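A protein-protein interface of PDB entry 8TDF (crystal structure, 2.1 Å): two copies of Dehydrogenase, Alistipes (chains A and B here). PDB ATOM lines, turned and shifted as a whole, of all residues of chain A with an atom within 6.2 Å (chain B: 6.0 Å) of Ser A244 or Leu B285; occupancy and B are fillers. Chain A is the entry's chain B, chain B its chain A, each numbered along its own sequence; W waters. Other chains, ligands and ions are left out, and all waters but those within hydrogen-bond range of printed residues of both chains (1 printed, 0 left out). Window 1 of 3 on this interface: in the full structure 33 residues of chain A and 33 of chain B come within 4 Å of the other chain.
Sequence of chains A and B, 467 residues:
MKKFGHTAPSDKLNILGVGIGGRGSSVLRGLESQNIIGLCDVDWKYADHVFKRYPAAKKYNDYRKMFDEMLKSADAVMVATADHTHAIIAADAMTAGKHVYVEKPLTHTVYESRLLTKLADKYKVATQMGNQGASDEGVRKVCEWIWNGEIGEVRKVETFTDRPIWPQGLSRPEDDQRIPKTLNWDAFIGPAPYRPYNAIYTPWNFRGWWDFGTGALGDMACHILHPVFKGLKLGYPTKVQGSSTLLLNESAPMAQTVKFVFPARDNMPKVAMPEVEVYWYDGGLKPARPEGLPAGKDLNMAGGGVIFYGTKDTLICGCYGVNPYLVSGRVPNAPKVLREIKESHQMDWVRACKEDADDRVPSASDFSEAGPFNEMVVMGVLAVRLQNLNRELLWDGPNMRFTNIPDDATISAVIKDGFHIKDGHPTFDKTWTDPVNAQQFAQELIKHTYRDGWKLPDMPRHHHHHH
The backbone NH (N) of Thr A245 is in hydrogen-bond range of the backbone carbonyl oxygen (O) of Ala A255, at 3.0 Å. OG of Ser A243 lies within hydrogen-bond range of OG1 of Thr A257, 2.9 Å away. The side-chain amide nitrogen (NE2) of Gln A387 lies within hydrogen-bond range of the side-chain hydroxyl (OG) of Ser A244 (2.9 Å).
OG of Ser A243 lies within hydrogen-bond range of N of Lys B286 (3.1 Å). O of Ser A244 lies close to O of Gly B284, at 3.3 Å.
Hydrophobic or aromatic side chains of chain B within 4 Å of the printed part of chain A: Ala B255 and Leu B285. Among the printed residues, 9 pairs touch across the chains. Among the printed residues, no Asp or Glu carboxylate lies within 4 Å of a Lys or Arg side-chain nitrogen of the other chain.
Water W1 lies within hydrogen-bond range of O of Lys B286 and OG of Ser A243.
Ser A244 touches just these residues of chain B: Gly B284 (3.2 Å) and Leu B285 (3.9 Å). Of the printed residues of chain B, Thr A257 touches Leu B285 (3.9 Å). Gln A387 touches none of the printed residues of chain B. Of the printed residues of chain A, Ala B255 touches Thr A245. Tyr B281 touches none of the printed residues of chain A. Printed residues of chain A within 4 Å of Gly B283: Thr A245. Of the printed residues of chain A, Gly B284 touches Ser A243 (3.8 Å) and Ser A244 (3.2 Å). Printed residues of chain A within 4 Å of Leu B285: Ser A243, Ser A244, Thr A257 and Leu A285. The nearest residue of chain B that does not touch Ser A244 is Gly B283 (4.1 Å). The nearest printed residue of chain B that does not touch Thr A245 is Gly B284 (4.5 Å).
Thr A257 touches Leu B285, but with the chains exchanged Leu A285 does not touch Thr B257 (4.2 Å). Leu B285 touches its own counterpart, Leu A285. Positions printed for both chains: 255, 256, 257 and 285. Of the 9 pairs that touch across the chains among the printed residues, 1 has its exchanged pair printed and touching as well.
CB of Ser A243 touches O of Gly B284, at 3.8 Å. CA of Leu B285 touches OG of Ser A243, 3.6 Å away. Ser A244 touches Leu B285 (O to N, 3.9 Å). Thr A245 touches Ala B255 (CG2 to CB, 3.7 Å). Gly B283 touches Thr A245 (O to CA, 3.4 Å). CG2 of Thr A257 touches CD2 of Leu B285 (3.9 Å). Leu B285 touches Leu A285.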
ATOM      1  N   GLY A 242      -9.115  19.922  21.545  1.00  0.00           N
ATOM      2  CA  GLY A 242      -9.754  20.972  22.318  1.00  0.00           C
ATOM      3  C   GLY A 242     -10.454  20.403  23.560  1.00  0.00           C
ATOM      4  O   GLY A 242     -10.729  19.218  23.648  1.00  0.00           O
ATOM      5  N   SER A 243     -10.723  21.279  24.519  1.00  0.00           N
ATOM      6  CA  SER A 243     -11.634  20.979  25.580  1.00  0.00           C
ATOM      7  C   SER A 243     -12.412  22.264  25.900  1.00  0.00           C
ATOM      8  O   SER A 243     -12.105  23.344  25.380  1.00  0.00           O
ATOM      9  CB  SER A 243     -10.917  20.420  26.836  1.00  0.00           C
ATOM     10  OG  SER A 243      -9.982  21.360  27.349  1.00  0.00           O
ATOM     11  N   SER A 244     -13.506  22.105  26.647  1.00  0.00           N
ATOM     12  CA  SER A 244     -14.380  23.236  26.875  1.00  0.00           C
ATOM     13  C   SER A 244     -15.159  23.017  28.150  1.00  0.00           C
ATOM     14  O   SER A 244     -15.171  21.945  28.660  1.00  0.00           O
ATOM     15  CB  SER A 244     -15.216  23.502  25.677  1.00  0.00           C
ATOM     16  OG  SER A 244     -16.170  22.522  25.537  1.00  0.00           O
ATOM     17  N   THR A 245     -15.804  24.031  28.617  1.00  0.00           N
ATOM     18  CA  THR A 245     -16.932  23.883  29.489  1.00  0.00           C
ATOM     19  C   THR A 245     -18.022  23.100  28.798  1.00  0.00           C
ATOM     20  O   THR A 245     -17.944  22.834  27.599  1.00  0.00           O
ATOM     21  CB  THR A 245     -17.408  25.280  29.945  1.00  0.00           C
ATOM     22  OG1 THR A 245     -17.743  26.189  28.861  1.00  0.00           O
ATOM     23  CG2 THR A 245     -16.345  25.957  30.779  1.00  0.00           C
ATOM     24  N   LEU A 246     -19.119  22.859  29.495  1.00  0.00           N
ATOM     25  CA  LEU A 246     -20.237  22.062  29.030  1.00  0.00           C
ATOM     26  C   LEU A 246     -20.512  22.317  27.522  1.00  0.00           C
ATOM     27  O   LEU A 246     -20.834  23.435  27.100  1.00  0.00           O
ATOM     28  CB  LEU A 246     -21.438  22.553  29.835  1.00  0.00           C
ATOM     29  CG  LEU A 246     -22.710  21.712  29.657  1.00  0.00           C
ATOM     30  CD1 LEU A 246     -22.494  20.318  30.128  1.00  0.00           C
ATOM     31  CD2 LEU A 246     -23.871  22.370  30.368  1.00  0.00           C
ATOM     32  N   LEU A 247     -20.361  21.273  26.738  1.00  0.00           N
ATOM     33  CA  LEU A 247     -20.564  21.278  25.326  1.00  0.00           C
ATOM     34  C   LEU A 247     -21.987  20.807  25.013  1.00  0.00           C
ATOM     35  O   LEU A 247     -22.372  19.629  25.193  1.00  0.00           O
ATOM     36  CB  LEU A 247     -19.558  20.278  24.760  1.00  0.00           C
ATOM     37  CG  LEU A 247     -19.647  20.150  23.246  1.00  0.00           C
ATOM     38  CD1 LEU A 247     -19.329  21.493  22.598  1.00  0.00           C
ATOM     39  CD2 LEU A 247     -18.678  19.086  22.749  1.00  0.00           C
ATOM     40  N   PRO A 253     -19.650  26.845  23.772  1.00  0.00           N
ATOM     41  CA  PRO A 253     -19.405  26.822  25.208  1.00  0.00           C
ATOM     42  C   PRO A 253     -18.928  28.178  25.764  1.00  0.00           C
ATOM     43  O   PRO A 253     -18.521  29.076  25.023  1.00  0.00           O
ATOM     44  CB  PRO A 253     -18.331  25.774  25.400  1.00  0.00           C
ATOM     45  CG  PRO A 253     -17.896  25.390  24.036  1.00  0.00           C
ATOM     46  CD  PRO A 253     -18.514  26.318  23.017  1.00  0.00           C
ATOM     47  N   ALA A 255     -16.362  28.709  27.545  1.00  0.00           N
ATOM     48  CA  ALA A 255     -14.911  28.809  27.512  1.00  0.00           C
ATOM     49  C   ALA A 255     -14.325  27.537  26.899  1.00  0.00           C
ATOM     50  O   ALA A 255     -14.864  26.431  27.073  1.00  0.00           O
ATOM     51  CB  ALA A 255     -14.343  29.050  28.904  1.00  0.00           C
ATOM     52  N   GLN A 256     -13.180  27.693  26.237  1.00  0.00           N
ATOM     53  CA  GLN A 256     -12.570  26.599  25.537  1.00  0.00           C
ATOM     54  C   GLN A 256     -11.077  26.817  25.423  1.00  0.00           C
ATOM     55  O   GLN A 256     -10.567  27.897  25.617  1.00  0.00           O
ATOM     56  CB  GLN A 256     -13.340  26.376  24.236  1.00  0.00           C
ATOM     57  CG  GLN A 256     -13.053  27.302  23.127  1.00  0.00           C
ATOM     58  CD  GLN A 256     -14.166  27.479  22.064  1.00  0.00           C
ATOM     59  OE1 GLN A 256     -15.152  26.764  21.763  1.00  0.00           O
ATOM     60  NE2 GLN A 256     -13.910  28.537  21.361  1.00  0.00           N
ATOM     61  N   THR A 257     -10.368  25.709  25.196  1.00  0.00           N
ATOM     62  CA  THR A 257      -8.935  25.641  24.917  1.00  0.00           C
ATOM     63  C   THR A 257      -8.719  24.757  23.691  1.00  0.00           C
ATOM     64  O   THR A 257      -9.459  23.822  23.458  1.00  0.00           O
ATOM     65  CB  THR A 257      -8.115  25.065  26.093  1.00  0.00           C
ATOM     66  OG1 THR A 257      -8.546  23.746  26.442  1.00  0.00           O
ATOM     67  CG2 THR A 257      -8.360  25.819  27.375  1.00  0.00           C
ATOM     68  N   LEU A 285     -10.109  32.345  30.443  1.00  0.00           N
ATOM     69  CA  LEU A 285      -8.873  31.587  30.589  1.00  0.00           C
ATOM     70  C   LEU A 285      -7.750  32.269  29.856  1.00  0.00           C
ATOM     71  O   LEU A 285      -7.916  32.876  28.781  1.00  0.00           O
ATOM     72  CB  LEU A 285      -9.034  30.194  30.021  1.00  0.00           C
ATOM     73  CG  LEU A 285     -10.273  29.482  30.550  1.00  0.00           C
ATOM     74  CD1 LEU A 285     -10.486  28.209  29.721  1.00  0.00           C
ATOM     75  CD2 LEU A 285     -10.084  29.174  32.039  1.00  0.00           C
ATOM     76  N   VAL A 384     -13.223  21.261  19.313  1.00  0.00           N
ATOM     77  CA  VAL A 384     -14.011  21.371  20.531  1.00  0.00           C
ATOM     78  C   VAL A 384     -15.205  20.434  20.444  1.00  0.00           C
ATOM     79  O   VAL A 384     -15.532  19.776  21.439  1.00  0.00           O
ATOM     80  CB  VAL A 384     -14.397  22.845  20.771  1.00  0.00           C
ATOM     81  CG1 VAL A 384     -15.461  23.059  21.806  1.00  0.00           C
ATOM     82  CG2 VAL A 384     -13.211  23.650  21.147  1.00  0.00           C
ATOM     83  N   GLN A 387     -14.431  16.645  21.200  1.00  0.00           N
ATOM     84  CA  GLN A 387     -13.590  16.369  22.335  1.00  0.00           C
ATOM     85  C   GLN A 387     -13.967  15.022  22.944  1.00  0.00           C
ATOM     86  O   GLN A 387     -13.132  14.466  23.574  1.00  0.00           O
ATOM     87  CB  GLN A 387     -13.734  17.476  23.407  1.00  0.00           C
ATOM     88  CG  GLN A 387     -15.165  17.693  23.850  1.00  0.00           C
ATOM     89  CD  GLN A 387     -15.312  18.826  24.841  1.00  0.00           C
ATOM     90  OE1 GLN A 387     -15.423  18.569  26.024  1.00  0.00           O
ATOM     91  NE2 GLN A 387     -15.393  20.041  24.352  1.00  0.00           N
ATOM     92  N   PHE B 160      -6.809  17.317  36.860  1.00  0.00           N
ATOM     93  CA  PHE B 160      -8.070  17.946  36.595  1.00  0.00           C
ATOM     94  C   PHE B 160      -9.204  17.134  37.139  1.00  0.00           C
ATOM     95  O   PHE B 160      -9.051  15.970  37.456  1.00  0.00           O
ATOM     96  CB  PHE B 160      -8.280  18.004  35.070  1.00  0.00           C
ATOM     97  CG  PHE B 160      -8.617  16.688  34.434  1.00  0.00           C
ATOM     98  CD1 PHE B 160      -7.634  15.755  34.228  1.00  0.00           C
ATOM     99  CD2 PHE B 160      -9.925  16.436  34.013  1.00  0.00           C
ATOM    100  CE1 PHE B 160      -7.953  14.511  33.642  1.00  0.00           C
ATOM    101  CE2 PHE B 160     -10.236  15.220  33.325  1.00  0.00           C
ATOM    102  CZ  PHE B 160      -9.270  14.244  33.211  1.00  0.00           C
ATOM    103  N   THR B 161     -10.360  17.761  37.191  1.00  0.00           N
ATOM    104  CA  THR B 161     -11.632  17.168  37.483  1.00  0.00           C
ATOM    105  C   THR B 161     -12.619  17.714  36.495  1.00  0.00           C
ATOM    106  O   THR B 161     -12.455  18.785  35.968  1.00  0.00           O
ATOM    107  CB  THR B 161     -12.046  17.489  38.932  1.00  0.00           C
ATOM    108  OG1 THR B 161     -13.280  16.818  39.179  1.00  0.00           O
ATOM    109  CG2 THR B 161     -12.231  18.951  39.097  1.00  0.00           C
ATOM    110  N   ALA B 255     -15.366  27.491  35.453  1.00  0.00           N
ATOM    111  CA  ALA B 255     -14.167  26.693  35.217  1.00  0.00           C
ATOM    112  C   ALA B 255     -12.928  27.520  35.529  1.00  0.00           C
ATOM    113  O   ALA B 255     -12.940  28.735  35.395  1.00  0.00           O
ATOM    114  CB  ALA B 255     -14.135  26.279  33.683  1.00  0.00           C
ATOM    115  N   GLN B 256     -11.844  26.834  35.848  1.00  0.00           N
ATOM    116  CA  GLN B 256     -10.643  27.466  36.296  1.00  0.00           C
ATOM    117  C   GLN B 256      -9.419  26.668  35.958  1.00  0.00           C
ATOM    118  O   GLN B 256      -9.523  25.452  35.663  1.00  0.00           O
ATOM    119  CB  GLN B 256     -10.824  27.846  37.766  1.00  0.00           C
ATOM    120  CG  GLN B 256     -10.719  26.788  38.741  1.00  0.00           C
ATOM    121  CD  GLN B 256     -11.383  27.162  40.077  1.00  0.00           C
ATOM    122  OE1 GLN B 256     -11.812  28.301  40.423  1.00  0.00           O
ATOM    123  NE2 GLN B 256     -11.536  26.094  40.830  1.00  0.00           N
ATOM    124  N   THR B 257      -8.292  27.371  35.881  1.00  0.00           N
ATOM    125  CA  THR B 257      -6.953  26.783  35.755  1.00  0.00           C
ATOM    126  C   THR B 257      -6.016  27.404  36.759  1.00  0.00           C
ATOM    127  O   THR B 257      -6.119  28.608  37.079  1.00  0.00           O
ATOM    128  CB  THR B 257      -6.298  27.043  34.385  1.00  0.00           C
ATOM    129  OG1 THR B 257      -6.182  28.476  34.137  1.00  0.00           O
ATOM    130  CG2 THR B 257      -7.141  26.406  33.319  1.00  0.00           C
ATOM    131  N   TYR B 281      -6.965  21.876  36.328  1.00  0.00           N
ATOM    132  CA  TYR B 281      -7.984  22.345  35.441  1.00  0.00           C
ATOM    133  C   TYR B 281      -9.304  21.787  35.948  1.00  0.00           C
ATOM    134  O   TYR B 281      -9.396  20.605  36.387  1.00  0.00           O
ATOM    135  CB  TYR B 281      -7.845  21.794  34.004  1.00  0.00           C
ATOM    136  CG  TYR B 281      -6.499  22.000  33.336  1.00  0.00           C
ATOM    137  CD1 TYR B 281      -5.421  21.215  33.699  1.00  0.00           C
ATOM    138  CD2 TYR B 281      -6.335  22.855  32.266  1.00  0.00           C
ATOM    139  CE1 TYR B 281      -4.200  21.330  33.073  1.00  0.00           C
ATOM    140  CE2 TYR B 281      -5.099  23.029  31.661  1.00  0.00           C
ATOM    141  CZ  TYR B 281      -4.028  22.301  32.130  1.00  0.00           C
ATOM    142  OH  TYR B 281      -2.788  22.353  31.611  1.00  0.00           O
ATOM    143  N   ASP B 282     -10.371  22.557  35.804  1.00  0.00           N
ATOM    144  CA  ASP B 282     -11.693  22.072  36.135  1.00  0.00           C
ATOM    145  C   ASP B 282     -12.786  22.646  35.248  1.00  0.00           C
ATOM    146  O   ASP B 282     -12.519  23.391  34.319  1.00  0.00           O
ATOM    147  CB  ASP B 282     -11.982  22.197  37.612  1.00  0.00           C
ATOM    148  CG  ASP B 282     -12.149  23.601  38.091  1.00  0.00           C
ATOM    149  OD1 ASP B 282     -12.791  24.391  37.281  1.00  0.00           O
ATOM    150  OD2 ASP B 282     -11.798  23.865  39.345  1.00  0.00           O
ATOM    151  N   GLY B 283     -14.007  22.142  35.437  1.00  0.00           N
ATOM    152  CA  GLY B 283     -15.214  22.623  34.794  1.00  0.00           C
ATOM    153  C   GLY B 283     -15.301  22.227  33.323  1.00  0.00           C
ATOM    154  O   GLY B 283     -16.023  22.851  32.570  1.00  0.00           O
ATOM    155  N   GLY B 284     -14.560  21.183  32.877  1.00  0.00           N
ATOM    156  CA  GLY B 284     -14.625  20.614  31.521  1.00  0.00           C
ATOM    157  C   GLY B 284     -13.246  20.694  30.888  1.00  0.00           C
ATOM    158  O   GLY B 284     -12.926  19.979  29.973  1.00  0.00           O
ATOM    159  N   LEU B 285     -12.418  21.619  31.362  1.00  0.00           N
ATOM    160  CA  LEU B 285     -11.120  21.792  30.762  1.00  0.00           C
ATOM    161  C   LEU B 285     -10.230  20.636  31.187  1.00  0.00           C
ATOM    162  O   LEU B 285     -10.338  20.109  32.324  1.00  0.00           O
ATOM    163  CB  LEU B 285     -10.527  23.099  31.267  1.00  0.00           C
ATOM    164  CG  LEU B 285     -11.403  24.297  30.945  1.00  0.00           C
ATOM    165  CD1 LEU B 285     -10.845  25.510  31.649  1.00  0.00           C
ATOM    166  CD2 LEU B 285     -11.378  24.496  29.483  1.00  0.00           C
ATOM    167  N   LYS B 286      -9.447  20.252  30.183  1.00  0.00           N
ATOM    168  CA  LYS B 286      -8.532  19.158  30.357  1.00  0.00           C
ATOM    169  C   LYS B 286      -7.150  19.570  29.900  1.00  0.00           C
ATOM    170  O   LYS B 286      -7.008  20.255  28.901  1.00  0.00           O
ATOM    171  CB  LYS B 286      -8.911  17.976  29.479  1.00  0.00           C
ATOM    172  CG  LYS B 286     -10.179  17.239  29.874  1.00  0.00           C
ATOM    173  CD  LYS B 286     -10.266  15.951  28.990  1.00  0.00           C
ATOM    174  CE  LYS B 286     -11.617  15.610  28.417  1.00  0.00           C
ATOM    175  NZ  LYS B 286     -12.543  15.599  29.564  1.00  0.00           N
ATOM    176  N   PRO B 287      -6.137  18.906  30.447  1.00  0.00           N
ATOM    177  CA  PRO B 287      -4.808  18.972  29.872  1.00  0.00           C
ATOM    178  C   PRO B 287      -4.752  18.263  28.532  1.00  0.00           C
ATOM    179  O   PRO B 287      -5.632  17.487  28.224  1.00  0.00           O
ATOM    180  CB  PRO B 287      -3.937  18.170  30.856  1.00  0.00           C
ATOM    181  CG  PRO B 287      -4.928  17.327  31.607  1.00  0.00           C
ATOM    182  CD  PRO B 287      -6.262  18.017  31.596  1.00  0.00           C
HETATM  183  O   HOH W   1      -7.446  19.901  26.349  1.00  0.00           O
